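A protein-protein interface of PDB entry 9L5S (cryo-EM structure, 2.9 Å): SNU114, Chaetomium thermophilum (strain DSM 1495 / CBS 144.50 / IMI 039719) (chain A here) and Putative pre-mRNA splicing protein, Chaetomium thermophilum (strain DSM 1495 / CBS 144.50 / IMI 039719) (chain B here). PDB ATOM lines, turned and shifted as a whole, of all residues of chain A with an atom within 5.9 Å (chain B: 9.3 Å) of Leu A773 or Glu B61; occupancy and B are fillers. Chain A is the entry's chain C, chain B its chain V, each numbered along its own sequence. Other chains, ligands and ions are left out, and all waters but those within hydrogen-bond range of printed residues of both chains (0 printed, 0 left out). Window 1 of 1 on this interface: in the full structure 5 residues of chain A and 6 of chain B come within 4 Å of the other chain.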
ATOM      1  N   GLU A 765      -9.086   3.369 -37.789  1.00  0.00           N
ATOM      2  CA  GLU A 765      -9.069   1.991 -37.302  1.00  0.00           C
ATOM      3  C   GLU A 765      -8.603   1.020 -38.380  1.00  0.00           C
ATOM      4  O   GLU A 765      -7.815   0.108 -38.100  1.00  0.00           O
ATOM      5  CB  GLU A 765     -10.451   1.580 -36.791  1.00  0.00           C
ATOM      6  CG  GLU A 765     -10.895   2.282 -35.522  1.00  0.00           C
ATOM      7  CD  GLU A 765      -9.990   1.999 -34.345  1.00  0.00           C
ATOM      8  OE1 GLU A 765      -9.584   0.832 -34.166  1.00  0.00           O
ATOM      9  OE2 GLU A 765      -9.683   2.953 -33.603  1.00  0.00           O
ATOM     10  N   ASP A 771      -7.014   3.659 -31.199  1.00  0.00           N
ATOM     11  CA  ASP A 771      -8.064   3.382 -30.228  1.00  0.00           C
ATOM     12  C   ASP A 771      -9.364   4.019 -30.702  1.00  0.00           C
ATOM     13  O   ASP A 771      -9.364   5.139 -31.221  1.00  0.00           O
ATOM     14  CB  ASP A 771      -7.678   3.911 -28.845  1.00  0.00           C
ATOM     15  CG  ASP A 771      -8.815   3.817 -27.842  1.00  0.00           C
ATOM     16  OD1 ASP A 771      -9.565   2.820 -27.875  1.00  0.00           O
ATOM     17  OD2 ASP A 771      -8.958   4.745 -27.018  1.00  0.00           O
ATOM     18  N   LYS A 772     -10.469   3.284 -30.536  1.00  0.00           N
ATOM     19  CA  LYS A 772     -11.759   3.734 -31.053  1.00  0.00           C
ATOM     20  C   LYS A 772     -12.238   5.001 -30.353  1.00  0.00           C
ATOM     21  O   LYS A 772     -12.777   5.907 -30.999  1.00  0.00           O
ATOM     22  CB  LYS A 772     -12.794   2.618 -30.916  1.00  0.00           C
ATOM     23  CG  LYS A 772     -12.557   1.446 -31.854  1.00  0.00           C
ATOM     24  CD  LYS A 772     -13.618   0.373 -31.682  1.00  0.00           C
ATOM     25  CE  LYS A 772     -13.350  -0.812 -32.594  1.00  0.00           C
ATOM     26  NZ  LYS A 772     -14.251  -1.958 -32.292  1.00  0.00           N
ATOM     27  N   LEU A 773     -12.055   5.082 -29.032  1.00  0.00           N
ATOM     28  CA  LEU A 773     -12.374   6.319 -28.325  1.00  0.00           C
ATOM     29  C   LEU A 773     -11.421   7.435 -28.734  1.00  0.00           C
ATOM     30  O   LEU A 773     -11.830   8.596 -28.844  1.00  0.00           O
ATOM     31  CB  LEU A 773     -12.351   6.083 -26.810  1.00  0.00           C
ATOM     32  CG  LEU A 773     -12.836   7.167 -25.833  1.00  0.00           C
ATOM     33  CD1 LEU A 773     -13.377   6.508 -24.580  1.00  0.00           C
ATOM     34  CD2 LEU A 773     -11.743   8.157 -25.433  1.00  0.00           C
ATOM     35  N   ALA A 774     -10.146   7.103 -28.954  1.00  0.00           N
ATOM     36  CA  ALA A 774      -9.202   8.089 -29.469  1.00  0.00           C
ATOM     37  C   ALA A 774      -9.564   8.518 -30.885  1.00  0.00           C
ATOM     38  O   ALA A 774      -9.431   9.698 -31.233  1.00  0.00           O
ATOM     39  CB  ALA A 774      -7.782   7.527 -29.427  1.00  0.00           C
ATOM     40  N   ALA A 775     -10.009   7.572 -31.717  1.00  0.00           N
ATOM     41  CA  ALA A 775     -10.411   7.901 -33.082  1.00  0.00           C
ATOM     42  C   ALA A 775     -11.650   8.787 -33.111  1.00  0.00           C
ATOM     43  O   ALA A 775     -11.733   9.705 -33.935  1.00  0.00           O
ATOM     44  CB  ALA A 775     -10.655   6.622 -33.883  1.00  0.00           C
ATOM     45  N   ARG A 776     -12.614   8.535 -32.229  1.00  0.00           N
ATOM     46  CA  ARG A 776     -13.793   9.382 -32.122  1.00  0.00           C
ATOM     47  C   ARG A 776     -13.528  10.668 -31.351  1.00  0.00           C
ATOM     48  O   ARG A 776     -14.362  11.579 -31.390  1.00  0.00           O
ATOM     49  CB  ARG A 776     -14.939   8.622 -31.446  1.00  0.00           C
ATOM     50  CG  ARG A 776     -15.522   7.488 -32.273  1.00  0.00           C
ATOM     51  CD  ARG A 776     -16.400   6.593 -31.414  1.00  0.00           C
ATOM     52  NE  ARG A 776     -16.879   5.424 -32.142  1.00  0.00           N
ATOM     53  CZ  ARG A 776     -17.678   4.499 -31.629  1.00  0.00           C
ATOM     54  NH1 ARG A 776     -18.111   4.574 -30.381  1.00  0.00           N
ATOM     55  NH2 ARG A 776     -18.051   3.471 -32.387  1.00  0.00           N
ATOM     56  N   SER A 777     -12.395  10.761 -30.659  1.00  0.00           N
ATOM     57  CA  SER A 777     -12.047  11.927 -29.863  1.00  0.00           C
ATOM     58  C   SER A 777     -11.062  12.849 -30.568  1.00  0.00           C
ATOM     59  O   SER A 777     -10.563  13.793 -29.948  1.00  0.00           O
ATOM     60  CB  SER A 777     -11.480  11.487 -28.513  1.00  0.00           C
ATOM     61  OG  SER A 777     -12.391  10.646 -27.828  1.00  0.00           O
ATOM     62  N   ILE A 778     -10.762  12.589 -31.839  1.00  0.00           N
ATOM     63  CA  ILE A 778      -9.925  13.489 -32.628  1.00  0.00           C
ATOM     64  C   ILE A 778     -10.726  14.764 -32.864  1.00  0.00           C
ATOM     65  O   ILE A 778     -11.718  14.757 -33.599  1.00  0.00           O
ATOM     66  CB  ILE A 778      -9.494  12.848 -33.951  1.00  0.00           C
ATOM     67  CG1 ILE A 778      -8.513  11.704 -33.703  1.00  0.00           C
ATOM     68  CG2 ILE A 778      -8.848  13.881 -34.865  1.00  0.00           C
ATOM     69  CD1 ILE A 778      -8.218  10.885 -34.938  1.00  0.00           C
ATOM     70  N   GLN A 792      -6.606  16.106 -30.145  1.00  0.00           N
ATOM     71  CA  GLN A 792      -7.408  14.941 -29.801  1.00  0.00           C
ATOM     72  C   GLN A 792      -7.615  14.864 -28.292  1.00  0.00           C
ATOM     73  O   GLN A 792      -6.705  15.164 -27.509  1.00  0.00           O
ATOM     74  CB  GLN A 792      -6.714  13.669 -30.321  1.00  0.00           C
ATOM     75  CG  GLN A 792      -7.257  12.350 -29.805  1.00  0.00           C
ATOM     76  CD  GLN A 792      -6.182  11.287 -29.722  1.00  0.00           C
ATOM     77  OE1 GLN A 792      -5.261  11.253 -30.538  1.00  0.00           O
ATOM     78  NE2 GLN A 792      -6.275  10.430 -28.714  1.00  0.00           N
ATOM     79  N   ASP A 793      -8.821  14.467 -27.890  1.00  0.00           N
ATOM     80  CA  ASP A 793      -9.130  14.211 -26.492  1.00  0.00           C
ATOM     81  C   ASP A 793      -8.602  12.844 -26.073  1.00  0.00           C
ATOM     82  O   ASP A 793      -8.686  11.872 -26.828  1.00  0.00           O
ATOM     83  CB  ASP A 793     -10.640  14.271 -26.255  1.00  0.00           C
ATOM     84  CG  ASP A 793     -11.037  13.793 -24.875  1.00  0.00           C
ATOM     85  OD1 ASP A 793     -10.735  14.503 -23.895  1.00  0.00           O
ATOM     86  OD2 ASP A 793     -11.647  12.707 -24.772  1.00  0.00           O
ATOM     87  N   ASP A 794      -8.046  12.781 -24.864  1.00  0.00           N
ATOM     88  CA  ASP A 794      -7.706  11.514 -24.231  1.00  0.00           C
ATOM     89  C   ASP A 794      -8.110  11.539 -22.757  1.00  0.00           C
ATOM     90  O   ASP A 794      -7.672  10.684 -21.978  1.00  0.00           O
ATOM     91  CB  ASP A 794      -6.206  11.217 -24.419  1.00  0.00           C
ATOM     92  CG  ASP A 794      -5.831   9.778 -24.090  1.00  0.00           C
ATOM     93  OD1 ASP A 794      -6.162   8.878 -24.891  1.00  0.00           O
ATOM     94  OD2 ASP A 794      -5.203   9.552 -23.035  1.00  0.00           O
ATOM     95  N   THR A 795      -8.956  12.489 -22.361  1.00  0.00           N
ATOM     96  CA  THR A 795      -9.422  12.582 -20.987  1.00  0.00           C
ATOM     97  C   THR A 795     -10.465  11.507 -20.694  1.00  0.00           C
ATOM     98  O   THR A 795     -10.872  10.731 -21.563  1.00  0.00           O
ATOM     99  CB  THR A 795     -10.026  13.959 -20.706  1.00  0.00           C
ATOM    100  OG1 THR A 795     -11.146  14.177 -21.574  1.00  0.00           O
ATOM    101  CG2 THR A 795      -9.007  15.051 -20.928  1.00  0.00           C
ATOM    102  N   LEU A 796     -10.903  11.476 -19.435  1.00  0.00           N
ATOM    103  CA  LEU A 796     -11.955  10.584 -18.988  1.00  0.00           C
ATOM    104  C   LEU A 796     -13.189  11.378 -18.580  1.00  0.00           C
ATOM    105  O   LEU A 796     -13.063  12.463 -18.000  1.00  0.00           O
ATOM    106  CB  LEU A 796     -11.491   9.731 -17.801  1.00  0.00           C
ATOM    107  CG  LEU A 796     -10.369   8.731 -18.076  1.00  0.00           C
ATOM    108  CD1 LEU A 796      -9.809   8.198 -16.768  1.00  0.00           C
ATOM    109  CD2 LEU A 796     -10.865   7.595 -18.956  1.00  0.00           C
ATOM    110  N   GLU B  53      -1.174   5.096 -15.759  1.00  0.00           N
ATOM    111  CA  GLU B  53      -2.573   5.109 -15.337  1.00  0.00           C
ATOM    112  C   GLU B  53      -3.493   5.516 -16.483  1.00  0.00           C
ATOM    113  O   GLU B  53      -4.577   4.942 -16.657  1.00  0.00           O
ATOM    114  CB  GLU B  53      -2.754   6.048 -14.144  1.00  0.00           C
ATOM    115  N   HIS B  54      -3.072   6.502 -17.282  1.00  0.00           N
ATOM    116  CA  HIS B  54      -3.845   6.908 -18.450  1.00  0.00           C
ATOM    117  C   HIS B  54      -3.899   5.799 -19.492  1.00  0.00           C
ATOM    118  O   HIS B  54      -4.926   5.615 -20.152  1.00  0.00           O
ATOM    119  CB  HIS B  54      -3.254   8.183 -19.052  1.00  0.00           C
ATOM    120  N   ASP B  55      -2.803   5.052 -19.656  1.00  0.00           N
ATOM    121  CA  ASP B  55      -2.798   3.918 -20.578  1.00  0.00           C
ATOM    122  C   ASP B  55      -3.742   2.815 -20.111  1.00  0.00           C
ATOM    123  O   ASP B  55      -4.446   2.208 -20.928  1.00  0.00           O
ATOM    124  CB  ASP B  55      -1.377   3.377 -20.734  1.00  0.00           C
ATOM    125  N   ARG B  56      -3.769   2.541 -18.803  1.00  0.00           N
ATOM    126  CA  ARG B  56      -4.700   1.549 -18.269  1.00  0.00           C
ATOM    127  C   ARG B  56      -6.148   1.997 -18.440  1.00  0.00           C
ATOM    128  O   ARG B  56      -7.023   1.190 -18.788  1.00  0.00           O
ATOM    129  CB  ARG B  56      -4.391   1.280 -16.797  1.00  0.00           C
ATOM    130  N   LYS B  57      -6.419   3.285 -18.204  1.00  0.00           N
ATOM    131  CA  LYS B  57      -7.762   3.819 -18.411  1.00  0.00           C
ATOM    132  C   LYS B  57      -8.162   3.760 -19.881  1.00  0.00           C
ATOM    133  O   LYS B  57      -9.319   3.469 -20.206  1.00  0.00           O
ATOM    134  CB  LYS B  57      -7.842   5.252 -17.889  1.00  0.00           C
ATOM    135  N   ARG B  58      -7.215   4.030 -20.783  1.00  0.00           N
ATOM    136  CA  ARG B  58      -7.489   3.940 -22.213  1.00  0.00           C
ATOM    137  C   ARG B  58      -7.747   2.501 -22.640  1.00  0.00           C
ATOM    138  O   ARG B  58      -8.590   2.251 -23.506  1.00  0.00           O
ATOM    139  CB  ARG B  58      -6.328   4.536 -23.008  1.00  0.00           C
ATOM    140  N   GLU B  59      -7.030   1.541 -22.049  1.00  0.00           N
ATOM    141  CA  GLU B  59      -7.289   0.132 -22.337  1.00  0.00           C
ATOM    142  C   GLU B  59      -8.669  -0.292 -21.845  1.00  0.00           C
ATOM    143  O   GLU B  59      -9.381  -1.033 -22.537  1.00  0.00           O
ATOM    144  CB  GLU B  59      -6.202  -0.739 -21.707  1.00  0.00           C
ATOM    145  N   VAL B  60      -9.063   0.173 -20.655  1.00  0.00           N
ATOM    146  CA  VAL B  60     -10.397  -0.127 -20.135  1.00  0.00           C
ATOM    147  C   VAL B  60     -11.473   0.494 -21.020  1.00  0.00           C
ATOM    148  O   VAL B  60     -12.503  -0.131 -21.307  1.00  0.00           O
ATOM    149  CB  VAL B  60     -10.520   0.349 -18.675  1.00  0.00           C
ATOM    150  N   GLU B  61     -11.246   1.730 -21.473  1.00  0.00           N
ATOM    151  CA  GLU B  61     -12.191   2.387 -22.370  1.00  0.00           C
ATOM    152  C   GLU B  61     -12.249   1.702 -23.731  1.00  0.00           C
ATOM    153  O   GLU B  61     -13.318   1.652 -24.347  1.00  0.00           O
ATOM    154  CB  GLU B  61     -11.818   3.860 -22.532  1.00  0.00           C
ATOM    155  N   VAL B  62     -11.123   1.167 -24.207  1.00  0.00           N
ATOM    156  CA  VAL B  62     -11.113   0.425 -25.464  1.00  0.00           C
ATOM    157  C   VAL B  62     -11.898  -0.872 -25.327  1.00  0.00           C
ATOM    158  O   VAL B  62     -12.626  -1.271 -26.243  1.00  0.00           O
ATOM    159  CB  VAL B  62      -9.665   0.162 -25.915  1.00  0.00           C
ATOM    160  N   LYS B  63     -11.758  -1.551 -24.185  1.00  0.00           N
ATOM    161  CA  LYS B  63     -12.552  -2.752 -23.931  1.00  0.00           C
ATOM    162  C   LYS B  63     -14.041  -2.424 -23.854  1.00  0.00           C
ATOM    163  O   LYS B  63     -14.879  -3.173 -24.374  1.00  0.00           O
ATOM    164  CB  LYS B  63     -12.083  -3.429 -22.645  1.00  0.00           C
ATOM    165  N   VAL B  64     -14.384  -1.299 -23.220  1.00  0.00           N
ATOM    166  CA  VAL B  64     -15.782  -0.876 -23.131  1.00  0.00           C
ATOM    167  C   VAL B  64     -16.333  -0.538 -24.513  1.00  0.00           C
ATOM    168  O   VAL B  64     -17.480  -0.867 -24.838  1.00  0.00           O
ATOM    169  CB  VAL B  64     -15.921   0.310 -22.160  1.00  0.00           C
ATOM    170  N   PHE B  65     -15.526   0.128 -25.345  1.00  0.00           N
ATOM    171  CA  PHE B  65     -15.957   0.467 -26.698  1.00  0.00           C
ATOM    172  C   PHE B  65     -16.117  -0.780 -27.559  1.00  0.00           C
ATOM    173  O   PHE B  65     -17.033  -0.856 -28.386  1.00  0.00           O
ATOM    174  CB  PHE B  65     -14.964   1.437 -27.337  1.00  0.00           C
ATOM    175  N   GLU B  66     -15.233  -1.766 -27.383  1.00  0.00           N
ATOM    176  CA  GLU B  66     -15.372  -3.030 -28.102  1.00  0.00           C
ATOM    177  C   GLU B  66     -16.632  -3.772 -27.675  1.00  0.00           C
ATOM    178  O   GLU B  66     -17.331  -4.354 -28.514  1.00  0.00           O
ATOM    179  CB  GLU B  66     -14.133  -3.898 -27.878  1.00  0.00           C
ATOM    180  N   LEU B  67     -16.939  -3.760 -26.374  1.00  0.00           N
ATOM    181  CA  LEU B  67     -18.173  -4.375 -25.893  1.00  0.00           C
ATOM    182  C   LEU B  67     -19.404  -3.656 -26.437  1.00  0.00           C
ATOM    183  O   LEU B  67     -20.394  -4.297 -26.807  1.00  0.00           O
ATOM    184  CB  LEU B  67     -18.192  -4.388 -24.365  1.00  0.00           C
ATOM    185  N   ARG B  68     -19.355  -2.321 -26.496  1.00  0.00           N
ATOM    186  CA  ARG B  68     -20.464  -1.553 -27.053  1.00  0.00           C
ATOM    187  C   ARG B  68     -20.644  -1.831 -28.542  1.00  0.00           C
ATOM    188  O   ARG B  68     -21.778  -1.930 -29.026  1.00  0.00           O
ATOM    189  CB  ARG B  68     -20.242  -0.060 -26.809  1.00  0.00           C
ATOM    190  N   ASP B  69     -19.540  -1.960 -29.282  1.00  0.00           N
ATOM    191  CA  ASP B  69     -19.624  -2.286 -30.703  1.00  0.00           C
ATOM    192  C   ASP B  69     -20.167  -3.694 -30.919  1.00  0.00           C
ATOM    193  O   ASP B  69     -20.932  -3.932 -31.863  1.00  0.00           O
ATOM    194  CB  ASP B  69     -18.253  -2.133 -31.359  1.00  0.00           C
ATOM    195  N   CYS B  85     -21.919  -1.899 -20.261  1.00  0.00           N
ATOM    196  CA  CYS B  85     -20.709  -1.088 -20.354  1.00  0.00           C
ATOM    197  C   CYS B  85     -20.323  -0.504 -19.000  1.00  0.00           C
ATOM    198  O   CYS B  85     -19.136  -0.455 -18.659  1.00  0.00           O
ATOM    199  CB  CYS B  85     -20.904   0.027 -21.383  1.00  0.00           C
ATOM    200  N   LEU B  88     -18.897  -3.364 -16.979  1.00  0.00           N
ATOM    201  CA  LEU B  88     -17.559  -3.687 -17.464  1.00  0.00           C
ATOM    202  C   LEU B  88     -16.541  -2.639 -17.032  1.00  0.00           C
ATOM    203  O   LEU B  88     -15.403  -2.981 -16.697  1.00  0.00           O
ATOM    204  CB  LEU B  88     -17.574  -3.826 -18.986  1.00  0.00           C
ATOM    205  N   ARG B  89     -16.929  -1.361 -17.037  1.00  0.00           N
ATOM    206  CA  ARG B  89     -16.034  -0.306 -16.571  1.00  0.00           C
ATOM    207  C   ARG B  89     -15.739  -0.445 -15.082  1.00  0.00           C
ATOM    208  O   ARG B  89     -14.592  -0.272 -14.650  1.00  0.00           O
ATOM    209  CB  ARG B  89     -16.637   1.066 -16.874  1.00  0.00           C
ATOM    210  N   LEU B  92     -13.403  -3.401 -14.690  1.00  0.00           N
ATOM    211  CA  LEU B  92     -12.056  -3.049 -15.125  1.00  0.00           C
ATOM    212  C   LEU B  92     -11.353  -2.167 -14.100  1.00  0.00           C
ATOM    213  O   LEU B  92     -10.154  -2.334 -13.852  1.00  0.00           O
ATOM    214  CB  LEU B  92     -12.108  -2.355 -16.485  1.00  0.00           C
ATOM    215  N   LEU B  93     -12.084  -1.225 -13.494  1.00  0.00           N
ATOM    216  CA  LEU B  93     -11.501  -0.394 -12.445  1.00  0.00           C
ATOM    217  C   LEU B  93     -11.124  -1.226 -11.223  1.00  0.00           C
ATOM    218  O   LEU B  93     -10.053  -1.027 -10.633  1.00  0.00           O
ATOM    219  CB  LEU B  93     -12.473   0.720 -12.057  1.00  0.00           C
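Among the printed residues, pairs that only touch across the chains: Asp A771 with Val B62 (3.3 Å), Leu A773 with Glu B61 (3.7 Å) and Leu A796 with Lys B57 (3.7 Å).
The side-chain carboxylate (OD2) of Asp A771 lies within hydrogen-bond range of the backbone NH (N) of Ala A774 (3.3 Å).
Of chain B, only Glu B61 comes within 4 Å of Leu A773. Of the printed residues of chain A, Glu B61 touches Leu A773 (3.7 Å). No residue of chain B comes within 4 Å of Ala A774. Printed residues of chain B within 4 Å of Asp A771: Val B62. Of the printed residues of chain A, Val B62 touches Asp A771. Printed residues of chain B within 4 Å of Leu A796: Lys B57 (3.7 Å). The nearest printed residue of chain B that does not touch Asp A771 is Arg B58 (4.3 Å).
Of the 14 printed residues of chain A, 3 touch a printed residue of chain B. Along chain A the printed residues that touch a printed residue of chain B span positions 771 to 796. Hydrophobic or aromatic side chains of chain B that line the printed part of chain A: Val B62.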
